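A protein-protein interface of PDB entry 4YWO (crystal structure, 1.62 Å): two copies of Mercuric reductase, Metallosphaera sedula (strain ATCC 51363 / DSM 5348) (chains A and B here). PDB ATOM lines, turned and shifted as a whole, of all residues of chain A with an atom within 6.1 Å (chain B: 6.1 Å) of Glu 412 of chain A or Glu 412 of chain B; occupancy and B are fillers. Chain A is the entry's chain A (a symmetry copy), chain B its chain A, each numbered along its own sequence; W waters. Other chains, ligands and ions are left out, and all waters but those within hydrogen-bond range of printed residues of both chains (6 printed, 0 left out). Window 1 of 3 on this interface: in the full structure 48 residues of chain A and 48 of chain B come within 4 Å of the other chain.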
ATOM      1  N   ASN A 350     -25.445  20.104 -19.721  1.00  0.00           N
ATOM      2  CA  ASN A 350     -24.389  20.483 -18.780  1.00  0.00           C
ATOM      3  C   ASN A 350     -23.742  21.838 -19.155  1.00  0.00           C
ATOM      4  O   ASN A 350     -23.762  22.292 -20.332  1.00  0.00           O
ATOM      5  CB  ASN A 350     -23.259  19.508 -18.773  1.00  0.00           C
ATOM      6  CG  ASN A 350     -23.537  18.074 -18.372  1.00  0.00           C
ATOM      7  OD1 ASN A 350     -22.721  17.192 -18.718  1.00  0.00           O
ATOM      8  ND2 ASN A 350     -24.653  17.775 -17.726  1.00  0.00           N
ATOM      9  N   LYS A 380     -23.169  15.565 -33.901  1.00  0.00           N
ATOM     10  CA  LYS A 380     -23.812  14.711 -32.940  1.00  0.00           C
ATOM     11  C   LYS A 380     -24.949  15.443 -32.198  1.00  0.00           C
ATOM     12  O   LYS A 380     -25.947  14.880 -31.832  1.00  0.00           O
ATOM     13  CB  LYS A 380     -22.778  14.145 -31.914  1.00  0.00           C
ATOM     14  CG  LYS A 380     -23.374  13.117 -30.960  1.00  0.00           C
ATOM     15  CD  LYS A 380     -24.023  11.949 -31.741  1.00  0.00           C
ATOM     16  CE  LYS A 380     -24.304  10.659 -31.001  1.00  0.00           C
ATOM     17  NZ  LYS A 380     -23.039   9.978 -30.606  1.00  0.00           N
ATOM     18  N   GLU A 408     -24.930  18.736 -24.370  1.00  0.00           N
ATOM     19  CA  GLU A 408     -25.290  17.433 -23.812  1.00  0.00           C
ATOM     20  C   GLU A 408     -24.013  16.681 -23.385  1.00  0.00           C
ATOM     21  O   GLU A 408     -23.138  16.386 -24.202  1.00  0.00           O
ATOM     22  CB  GLU A 408     -25.992  16.577 -24.900  1.00  0.00           C
ATOM     23  CG  GLU A 408     -26.849  15.509 -24.300  1.00  0.00           C
ATOM     24  CD  GLU A 408     -28.060  16.117 -23.516  1.00  0.00           C
ATOM     25  OE1 GLU A 408     -28.279  15.478 -22.508  1.00  0.00           O
ATOM     26  OE2 GLU A 408     -28.680  17.241 -23.827  1.00  0.00           O
ATOM     27  N   ASN A 409     -23.926  16.333 -22.117  1.00  0.00           N
ATOM     28  CA  ASN A 409     -22.855  15.557 -21.559  1.00  0.00           C
ATOM     29  C   ASN A 409     -21.491  16.183 -21.788  1.00  0.00           C
ATOM     30  O   ASN A 409     -20.494  15.487 -21.801  1.00  0.00           O
ATOM     31  CB  ASN A 409     -22.834  14.159 -22.136  1.00  0.00           C
ATOM     32  CG  ASN A 409     -24.073  13.353 -21.814  1.00  0.00           C
ATOM     33  OD1 ASN A 409     -24.566  12.595 -22.714  1.00  0.00           O
ATOM     34  ND2 ASN A 409     -24.541  13.421 -20.595  1.00  0.00           N
ATOM     35  N   VAL A 410     -21.422  17.545 -21.867  1.00  0.00           N
ATOM     36  CA  VAL A 410     -20.087  18.168 -22.003  1.00  0.00           C
ATOM     37  C   VAL A 410     -19.211  17.903 -20.771  1.00  0.00           C
ATOM     38  O   VAL A 410     -18.018  18.113 -20.833  1.00  0.00           O
ATOM     39  CB  VAL A 410     -20.163  19.628 -22.454  1.00  0.00           C
ATOM     40  CG1 VAL A 410     -20.764  19.789 -23.832  1.00  0.00           C
ATOM     41  CG2 VAL A 410     -20.865  20.540 -21.449  1.00  0.00           C
ATOM     42  N   ALA A 411     -19.798  17.519 -19.645  1.00  0.00           N
ATOM     43  CA  ALA A 411     -18.969  17.117 -18.539  1.00  0.00           C
ATOM     44  C   ALA A 411     -17.951  16.019 -18.882  1.00  0.00           C
ATOM     45  O   ALA A 411     -16.854  16.018 -18.297  1.00  0.00           O
ATOM     46  CB  ALA A 411     -19.823  16.586 -17.422  1.00  0.00           C
ATOM     47  N   GLU A 412     -18.250  15.207 -19.892  1.00  0.00           N
ATOM     48  CA  GLU A 412     -17.442  14.035 -20.266  1.00  0.00           C
ATOM     49  C   GLU A 412     -16.263  14.439 -21.122  1.00  0.00           C
ATOM     50  O   GLU A 412     -15.354  13.624 -21.271  1.00  0.00           O
ATOM     51  CB  GLU A 412     -18.276  12.937 -20.924  1.00  0.00           C
ATOM     52  CG  GLU A 412     -19.344  12.344 -20.028  1.00  0.00           C
ATOM     53  CD  GLU A 412     -18.807  11.607 -18.765  1.00  0.00           C
ATOM     54  OE1 GLU A 412     -17.562  11.398 -18.768  1.00  0.00           O
ATOM     55  OE2 GLU A 412     -19.559  11.379 -17.750  1.00  0.00           O
ATOM     56  N   MET A 413     -16.329  15.586 -21.786  1.00  0.00           N
ATOM     57  CA  MET A 413     -15.236  16.088 -22.627  1.00  0.00           C
ATOM     58  C   MET A 413     -14.347  17.111 -21.925  1.00  0.00           C
ATOM     59  O   MET A 413     -13.272  17.432 -22.423  1.00  0.00           O
ATOM     60  CB  MET A 413     -15.731  16.737 -23.917  1.00  0.00           C
ATOM     61  CG  MET A 413     -16.252  18.136 -23.764  1.00  0.00           C
ATOM     62  SD  MET A 413     -16.965  18.647 -25.369  1.00  0.00           S
ATOM     63  CE  MET A 413     -17.176  20.412 -25.139  1.00  0.00           C
ATOM     64  N   ILE A 414     -14.719  17.605 -20.754  1.00  0.00           N
ATOM     65  CA  ILE A 414     -13.976  18.702 -20.127  1.00  0.00           C
ATOM     66  C   ILE A 414     -12.669  18.173 -19.604  1.00  0.00           C
ATOM     67  O   ILE A 414     -11.697  18.932 -19.507  1.00  0.00           O
ATOM     68  CB  ILE A 414     -14.812  19.449 -19.076  1.00  0.00           C
ATOM     69  CG1 ILE A 414     -14.346  20.920 -18.906  1.00  0.00           C
ATOM     70  CG2 ILE A 414     -14.863  18.713 -17.733  1.00  0.00           C
ATOM     71  CD1 ILE A 414     -14.570  21.770 -20.102  1.00  0.00           C
ATOM     72  N   GLY A 415     -12.528  16.840 -19.367  1.00  0.00           N
ATOM     73  CA  GLY A 415     -11.255  16.344 -18.965  1.00  0.00           C
ATOM     74  C   GLY A 415     -10.248  16.332 -20.134  1.00  0.00           C
ATOM     75  O   GLY A 415      -9.044  16.525 -19.875  1.00  0.00           O
ATOM     76  N   GLU A 416     -10.716  16.130 -21.352  1.00  0.00           N
ATOM     77  CA  GLU A 416      -9.820  16.340 -22.498  1.00  0.00           C
ATOM     78  C   GLU A 416      -9.291  17.742 -22.533  1.00  0.00           C
ATOM     79  O   GLU A 416      -8.061  17.954 -22.771  1.00  0.00           O
ATOM     80  CB  GLU A 416     -10.495  15.959 -23.795  1.00  0.00           C
ATOM     81  CG  GLU A 416      -9.660  16.131 -25.023  1.00  0.00           C
ATOM     82  CD  GLU A 416     -10.275  15.794 -26.377  1.00  0.00           C
ATOM     83  OE1 GLU A 416     -11.336  15.100 -26.455  1.00  0.00           O
ATOM     84  OE2 GLU A 416      -9.749  16.340 -27.416  1.00  0.00           O
ATOM     85  N   PRO A 438     -19.628  10.447 -34.906  1.00  0.00           N
ATOM     86  CA  PRO A 438     -20.037  11.801 -34.463  1.00  0.00           C
ATOM     87  C   PRO A 438     -20.114  11.726 -32.933  1.00  0.00           C
ATOM     88  O   PRO A 438     -20.882  10.885 -32.356  1.00  0.00           O
ATOM     89  CB  PRO A 438     -21.401  11.956 -35.098  1.00  0.00           C
ATOM     90  CG  PRO A 438     -21.928  10.542 -35.197  1.00  0.00           C
ATOM     91  CD  PRO A 438     -20.772   9.582 -35.148  1.00  0.00           C
ATOM     92  N   THR A 439     -19.387  12.604 -32.271  1.00  0.00           N
ATOM     93  CA  THR A 439     -19.409  12.780 -30.807  1.00  0.00           C
ATOM     94  C   THR A 439     -19.578  14.215 -30.482  1.00  0.00           C
ATOM     95  O   THR A 439     -19.218  15.097 -31.272  1.00  0.00           O
ATOM     96  CB  THR A 439     -18.146  12.216 -30.108  1.00  0.00           C
ATOM     97  OG1 THR A 439     -16.921  12.834 -30.607  1.00  0.00           O
ATOM     98  CG2 THR A 439     -18.088  10.686 -30.281  1.00  0.00           C
ATOM     99  N   ILE A 440     -20.038  14.487 -29.273  1.00  0.00           N
ATOM    100  CA  ILE A 440     -20.003  15.911 -28.776  1.00  0.00           C
ATOM    101  C   ILE A 440     -18.567  16.395 -28.597  1.00  0.00           C
ATOM    102  O   ILE A 440     -18.276  17.538 -28.899  1.00  0.00           O
ATOM    103  CB  ILE A 440     -20.861  16.043 -27.522  1.00  0.00           C
ATOM    104  CG1 ILE A 440     -22.367  15.642 -27.779  1.00  0.00           C
ATOM    105  CG2 ILE A 440     -20.768  17.506 -26.972  1.00  0.00           C
ATOM    106  CD1 ILE A 440     -23.075  16.561 -28.713  1.00  0.00           C
ATOM    107  N   ALA A 441     -17.691  15.518 -28.172  1.00  0.00           N
ATOM    108  CA  ALA A 441     -16.287  15.862 -27.916  1.00  0.00           C
ATOM    109  C   ALA A 441     -15.543  16.386 -29.120  1.00  0.00           C
ATOM    110  O   ALA A 441     -14.567  17.156 -28.989  1.00  0.00           O
ATOM    111  CB  ALA A 441     -15.592  14.727 -27.289  1.00  0.00           C
ATOM    112  N   GLU A 442     -15.928  15.954 -30.310  1.00  0.00           N
ATOM    113  CA  GLU A 442     -15.187  16.524 -31.435  1.00  0.00           C
ATOM    114  C   GLU A 442     -15.440  18.002 -31.617  1.00  0.00           C
ATOM    115  O   GLU A 442     -14.613  18.663 -32.317  1.00  0.00           O
ATOM    116  CB  GLU A 442     -15.453  15.921 -32.808  1.00  0.00           C
ATOM    117  CG  GLU A 442     -16.059  14.641 -32.918  1.00  0.00           C
ATOM    118  CD  GLU A 442     -16.682  14.441 -34.286  1.00  0.00           C
ATOM    119  OE1 GLU A 442     -15.960  14.330 -35.305  1.00  0.00           O
ATOM    120  OE2 GLU A 442     -17.902  14.312 -34.377  1.00  0.00           O
ATOM    121  N   ASN B 350     -21.660   2.129 -24.903  1.00  0.00           N
ATOM    122  CA  ASN B 350     -20.669   2.220 -25.978  1.00  0.00           C
ATOM    123  C   ASN B 350     -19.457   1.291 -25.724  1.00  0.00           C
ATOM    124  O   ASN B 350     -19.132   0.907 -24.566  1.00  0.00           O
ATOM    125  CB  ASN B 350     -20.085   3.588 -26.096  1.00  0.00           C
ATOM    126  CG  ASN B 350     -21.004   4.747 -26.419  1.00  0.00           C
ATOM    127  OD1 ASN B 350     -20.617   5.905 -26.151  1.00  0.00           O
ATOM    128  ND2 ASN B 350     -22.210   4.513 -26.914  1.00  0.00           N
ATOM    129  N   LYS B 380     -19.848   7.606 -10.989  1.00  0.00           N
ATOM    130  CA  LYS B 380     -20.911   8.068 -11.839  1.00  0.00           C
ATOM    131  C   LYS B 380     -21.699   6.895 -12.456  1.00  0.00           C
ATOM    132  O   LYS B 380     -22.880   6.958 -12.679  1.00  0.00           O
ATOM    133  CB  LYS B 380     -20.360   8.998 -12.968  1.00  0.00           C
ATOM    134  CG  LYS B 380     -21.457   9.638 -13.812  1.00  0.00           C
ATOM    135  CD  LYS B 380     -22.446  10.430 -12.925  1.00  0.00           C
ATOM    136  CE  LYS B 380     -23.349  11.448 -13.587  1.00  0.00           C
ATOM    137  NZ  LYS B 380     -22.564  12.600 -14.116  1.00  0.00           N
ATOM    138  N   GLU B 408     -21.220   3.716 -20.316  1.00  0.00           N
ATOM    139  CA  GLU B 408     -22.175   4.717 -20.788  1.00  0.00           C
ATOM    140  C   GLU B 408     -21.415   5.937 -21.348  1.00  0.00           C
ATOM    141  O   GLU B 408     -20.662   6.606 -20.638  1.00  0.00           O
ATOM    142  CB  GLU B 408     -23.039   5.214 -19.598  1.00  0.00           C
ATOM    143  CG  GLU B 408     -24.341   5.787 -20.058  1.00  0.00           C
ATOM    144  CD  GLU B 408     -25.255   4.691 -20.702  1.00  0.00           C
ATOM    145  OE1 GLU B 408     -25.852   5.142 -21.658  1.00  0.00           O
ATOM    146  OE2 GLU B 408     -25.282   3.418 -20.350  1.00  0.00           O
ATOM    147  N   ASN B 409     -21.646   6.252 -22.607  1.00  0.00           N
ATOM    148  CA  ASN B 409     -21.095   7.400 -23.271  1.00  0.00           C
ATOM    149  C   ASN B 409     -19.578   7.435 -23.230  1.00  0.00           C
ATOM    150  O   ASN B 409     -18.989   8.495 -23.320  1.00  0.00           O
ATOM    151  CB  ASN B 409     -21.612   8.684 -22.662  1.00  0.00           C
ATOM    152  CG  ASN B 409     -23.108   8.862 -22.805  1.00  0.00           C
ATOM    153  OD1 ASN B 409     -23.765   9.357 -21.830  1.00  0.00           O
ATOM    154  ND2 ASN B 409     -23.646   8.564 -23.958  1.00  0.00           N
ATOM    155  N   VAL B 410     -18.915   6.241 -23.199  1.00  0.00           N
ATOM    156  CA  VAL B 410     -17.437   6.263 -23.246  1.00  0.00           C
ATOM    157  C   VAL B 410     -16.922   6.847 -24.569  1.00  0.00           C
ATOM    158  O   VAL B 410     -15.759   7.178 -24.660  1.00  0.00           O
ATOM    159  CB  VAL B 410     -16.815   4.928 -22.831  1.00  0.00           C
ATOM    160  CG1 VAL B 410     -17.112   4.562 -21.394  1.00  0.00           C
ATOM    161  CG2 VAL B 410     -17.170   3.774 -23.767  1.00  0.00           C
ATOM    162  N   ALA B 411     -17.751   6.906 -25.603  1.00  0.00           N
ATOM    163  CA  ALA B 411     -17.323   7.597 -26.790  1.00  0.00           C
ATOM    164  C   ALA B 411     -16.849   9.037 -26.545  1.00  0.00           C
ATOM    165  O   ALA B 411     -15.943   9.498 -27.261  1.00  0.00           O
ATOM    166  CB  ALA B 411     -18.454   7.672 -27.778  1.00  0.00           C
ATOM    167  N   GLU B 412     -17.344   9.667 -25.483  1.00  0.00           N
ATOM    168  CA  GLU B 412     -17.086  11.083 -25.178  1.00  0.00           C
ATOM    169  C   GLU B 412     -15.753  11.256 -24.487  1.00  0.00           C
ATOM    170  O   GLU B 412     -15.277  12.388 -24.428  1.00  0.00           O
ATOM    171  CB  GLU B 412     -18.225  11.729 -24.391  1.00  0.00           C
ATOM    172  CG  GLU B 412     -19.546  11.773 -25.131  1.00  0.00           C
ATOM    173  CD  GLU B 412     -19.543  12.634 -26.430  1.00  0.00           C
ATOM    174  OE1 GLU B 412     -18.522  13.363 -26.574  1.00  0.00           O
ATOM    175  OE2 GLU B 412     -20.438  12.485 -27.338  1.00  0.00           O
ATOM    176  N   MET B 413     -15.231  10.213 -23.852  1.00  0.00           N
ATOM    177  CA  MET B 413     -13.934  10.260 -23.167  1.00  0.00           C
ATOM    178  C   MET B 413     -12.783   9.705 -24.002  1.00  0.00           C
ATOM    179  O   MET B 413     -11.624   9.897 -23.650  1.00  0.00           O
ATOM    180  CB  MET B 413     -13.935   9.497 -21.845  1.00  0.00           C
ATOM    181  CG  MET B 413     -13.811   8.007 -21.972  1.00  0.00           C
ATOM    182  SD  MET B 413     -14.028   7.282 -20.306  1.00  0.00           S
ATOM    183  CE  MET B 413     -13.478   5.595 -20.558  1.00  0.00           C
ATOM    184  N   ILE B 414     -13.045   9.065 -25.132  1.00  0.00           N
ATOM    185  CA  ILE B 414     -11.984   8.382 -25.876  1.00  0.00           C
ATOM    186  C   ILE B 414     -11.112   9.411 -26.542  1.00  0.00           C
ATOM    187  O   ILE B 414      -9.927   9.147 -26.779  1.00  0.00           O
ATOM    188  CB  ILE B 414     -12.535   7.317 -26.837  1.00  0.00           C
ATOM    189  CG1 ILE B 414     -11.502   6.191 -27.105  1.00  0.00           C
ATOM    190  CG2 ILE B 414     -13.066   7.919 -28.142  1.00  0.00           C
ATOM    191  CD1 ILE B 414     -11.184   5.361 -25.915  1.00  0.00           C
ATOM    192  N   GLY B 415     -11.594  10.666 -26.756  1.00  0.00           N
ATOM    193  CA  GLY B 415     -10.723  11.654 -27.298  1.00  0.00           C
ATOM    194  C   GLY B 415      -9.685  12.134 -26.263  1.00  0.00           C
ATOM    195  O   GLY B 415      -8.559  12.476 -26.674  1.00  0.00           O
ATOM    196  N   GLU B 416     -10.040  12.148 -24.991  1.00  0.00           N
ATOM    197  CA  GLU B 416      -9.008  12.380 -23.971  1.00  0.00           C
ATOM    198  C   GLU B 416      -7.923  11.349 -24.042  1.00  0.00           C
ATOM    199  O   GLU B 416      -6.703  11.699 -23.963  1.00  0.00           O
ATOM    200  CB  GLU B 416      -9.615  12.468 -22.590  1.00  0.00           C
ATOM    201  CG  GLU B 416      -8.643  12.710 -21.480  1.00  0.00           C
ATOM    202  CD  GLU B 416      -9.172  12.785 -20.051  1.00  0.00           C
ATOM    203  OE1 GLU B 416     -10.410  12.951 -19.823  1.00  0.00           O
ATOM    204  OE2 GLU B 416      -8.338  12.551 -19.101  1.00  0.00           O
ATOM    205  N   PRO B 438     -18.786  13.780 -10.285  1.00  0.00           N
ATOM    206  CA  PRO B 438     -18.617  12.371 -10.713  1.00  0.00           C
ATOM    207  C   PRO B 438     -18.908  12.361 -12.219  1.00  0.00           C
ATOM    208  O   PRO B 438     -20.030  12.769 -12.672  1.00  0.00           O
ATOM    209  CB  PRO B 438     -19.689  11.657  -9.918  1.00  0.00           C
ATOM    210  CG  PRO B 438     -20.761  12.705  -9.715  1.00  0.00           C
ATOM    211  CD  PRO B 438     -20.153  14.069  -9.879  1.00  0.00           C
ATOM    212  N   THR B 439     -17.960  11.868 -12.990  1.00  0.00           N
ATOM    213  CA  THR B 439     -18.084  11.659 -14.444  1.00  0.00           C
ATOM    214  C   THR B 439     -17.652  10.283 -14.786  1.00  0.00           C
ATOM    215  O   THR B 439     -16.850   9.668 -14.072  1.00  0.00           O
ATOM    216  CB  THR B 439     -17.288  12.695 -15.277  1.00  0.00           C
ATOM    217  OG1 THR B 439     -15.865  12.684 -14.951  1.00  0.00           O
ATOM    218  CG2 THR B 439     -17.879  14.102 -15.069  1.00  0.00           C
ATOM    219  N   ILE B 440     -18.094   9.805 -15.937  1.00  0.00           N
ATOM    220  CA  ILE B 440     -17.505   8.524 -16.474  1.00  0.00           C
ATOM    221  C   ILE B 440     -16.036   8.707 -16.843  1.00  0.00           C
ATOM    222  O   ILE B 440     -15.242   7.812 -16.611  1.00  0.00           O
ATOM    223  CB  ILE B 440     -18.369   7.997 -17.615  1.00  0.00           C
ATOM    224  CG1 ILE B 440     -19.855   7.711 -17.164  1.00  0.00           C
ATOM    225  CG2 ILE B 440     -17.719   6.705 -18.214  1.00  0.00           C
ATOM    226  CD1 ILE B 440     -19.972   6.603 -16.175  1.00  0.00           C
ATOM    227  N   ALA B 441     -15.687   9.864 -17.347  1.00  0.00           N
ATOM    228  CA  ALA B 441     -14.317  10.156 -17.784  1.00  0.00           C
ATOM    229  C   ALA B 441     -13.277  10.042 -16.697  1.00  0.00           C
ATOM    230  O   ALA B 441     -12.088   9.769 -16.969  1.00  0.00           O
ATOM    231  CB  ALA B 441     -14.267  11.462 -18.460  1.00  0.00           C
ATOM    232  N   GLU B 442     -13.661  10.298 -15.456  1.00  0.00           N
ATOM    233  CA  GLU B 442     -12.614  10.138 -14.448  1.00  0.00           C
ATOM    234  C   GLU B 442     -12.175   8.703 -14.278  1.00  0.00           C
ATOM    235  O   GLU B 442     -11.063   8.486 -13.705  1.00  0.00           O
ATOM    236  CB  GLU B 442     -12.943  10.604 -13.036  1.00  0.00           C
ATOM    237  CG  GLU B 442     -14.026  11.497 -12.817  1.00  0.00           C
ATOM    238  CD  GLU B 442     -14.500  11.445 -11.377  1.00  0.00           C
ATOM    239  OE1 GLU B 442     -13.778  11.888 -10.452  1.00  0.00           O
ATOM    240  OE2 GLU B 442     -15.633  11.034 -11.132  1.00  0.00           O
HETATM  241  O   HOH W   1     -18.681  15.290 -24.199  1.00  0.00           O
HETATM  242  O   HOH W   2     -17.160   9.528 -21.159  1.00  0.00           O
HETATM  243  O   HOH W   3     -21.437  10.368 -28.384  1.00  0.00           O
HETATM  244  O   HOH W   4     -21.240  12.881 -16.529  1.00  0.00           O
HETATM  245  O   HOH W   5     -12.729  13.919 -20.911  1.00  0.00           O
HETATM  246  O   HOH W   6     -12.850  13.253 -25.117  1.00  0.00           O
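Of the 16 printed residues of chain A, 8 touch a printed residue of chain B.
Printed residues of chain B that touch a printed residue of chain A: Asn 409, Ala 411, Glu 412, Gly 415, Glu 416, Thr 439, Ile 440 and Ala 441.
Hydrophobic or aromatic side chains of chain B within 4 Å of the printed part of chain A: Ala 411, Ile 440 and Ala 441.
Among the printed residues, 13 pairs touch across the chains.
Asn 409 of chain B touches its own counterpart, Asn 409 of chain A.
Ala 411 of chain A touches Thr 439 of chain B, and with the chains exchanged Thr 439 of chain A touches Ala 411 of chain B.
Glu 412 of chain A touches Thr 439 of chain B, and with the chains exchanged Thr 439 of chain A touches Glu 412 of chain B.
Gly 415 of chain A touches Glu 416 of chain B, and with the chains exchanged Glu 416 of chain A touches Gly 415 of chain B.
Positions printed for both chains: 350, 380, 408, 409, 410, 411, 412, 413, 414, 415, 416, 438, 439, 440, 441 and 442.
Of the 13 pairs that touch across the chains among the printed residues, 13 have their exchanged pair printed and touching as well.
Water W3 bridges the side-chain carboxylate (OE2) of Glu 412 of chain B (2.6 Å) and the side-chain amino group (NZ) of Lys 380 of chain A (2.8 Å).
Water W4 lies within hydrogen-bond range of OE2 of Glu 412 of chain A (2.6 Å) and NZ of Lys 380 of chain B (2.8 Å).
Water W6 lies within hydrogen-bond range of the backbone carbonyl oxygen (O) of Glu 412 of chain B (2.7 Å), the side-chain carboxylate (OE1) of Glu 416 of chain A (2.7 Å), the backbone NH (N) of Glu 416 of chain B (3.0 Å) and the backbone NH (N) of Gly 415 of chain B (3.3 Å).
Water W5 lies within hydrogen-bond range of the backbone carbonyl oxygen of Glu 412 of chain A, the side-chain carboxylate of Glu 416 of chain B, the backbone NH of Glu 416 of chain A and the backbone NH of Gly 415 of chain A.
Water W2 lies within hydrogen-bond range of the backbone carbonyl oxygen (O) of Asn 409 of chain B (3.0 Å), the side-chain carboxylate (OE1) of Glu 412 of chain A (3.1 Å) and the backbone NH (N) of Met 413 of chain B (3.4 Å).
Water W1 lies within hydrogen-bond range of the backbone carbonyl oxygen of Asn 409 of chain A (3.0 Å), the side-chain carboxylate of Glu 412 of chain B (3.1 Å) and the backbone NH of Met 413 of chain A (3.4 Å).
OD1 of Asn 350 of chain B lies within hydrogen-bond range of N of Ala 411 of chain B (3.1 Å).
N of Thr 439 of chain B sits at hydrogen-bond distance from OE2 of Glu 442 of chain B (3.1 Å).
OD1 of Asn 350 of chain A sits at hydrogen-bond distance from N of Ala 411 of chain A, at 3.1 Å.
The backbone NH (N) of Thr 439 of chain A is in hydrogen-bond range of the side-chain carboxylate (OE2) of Glu 442 of chain A, at 3.1 Å.
CG2 of Thr 439 of chain B touches O of Ala 411 of chain A, at 3.9 Å.
Thr 439 of chain B touches Glu 412 of chain A (CB to OE2, 3.6 Å).
Gly 415 of chain A touches Glu 416 of chain B (C to OE1, 3.4 Å).
OE1 of Glu 416 of chain A touches C of Gly 415 of chain B, 3.4 Å away.
N of Glu 416 of chain B touches OE1 of Glu 416 of chain A, 3.5 Å away.
Ala 411 of chain B touches Thr 439 of chain A.
Glu 412 of chain B touches Thr 439 of chain A.
OD1 of Asn 409 of chain B lies close to OD1 of Asn 409 of chain A (3.5 Å).
The side-chain carboxylate of Glu 412 of chain B is in hydrogen-bond range of the backbone NH of Ile 440 of chain A (2.8 Å).
The side-chain carboxylate (OE1) of Glu 412 of chain B lies within hydrogen-bond range of the backbone NH (N) of Ala 441 of chain A (2.8 Å).
The backbone NH (N) of Ile 440 of chain B is in hydrogen-bond range of the side-chain carboxylate (OE2) of Glu 412 of chain A.
The side-chain carboxylate (OE1) of Glu 412 of chain A lies within hydrogen-bond range of the backbone NH (N) of Ala 441 of chain B, 2.8 Å away.
The backbone carbonyl oxygen (O) of Glu 412 of chain A lies close to the backbone carbonyl oxygen (O) of Glu 412 of chain B, at 3.4 Å.
Of the printed residues of chain B, Glu 412 of chain A touches Glu 412 (3.4 Å), Thr 439 (3.6 Å), Ile 440 (2.8 Å) and Ala 441 (2.8 Å).
Of the printed residues of chain A, Glu 412 of chain B touches Glu 412, Thr 439, Ile 440 and Ala 441.
Printed residues of chain A within 4 Å of Ala 441 of chain B: Glu 412.
Of the printed residues of chain A, Thr 439 of chain B touches Ala 411 (3.9 Å) and Glu 412 (3.6 Å).
Lys 380 of chain B touches none of the printed residues of chain A.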
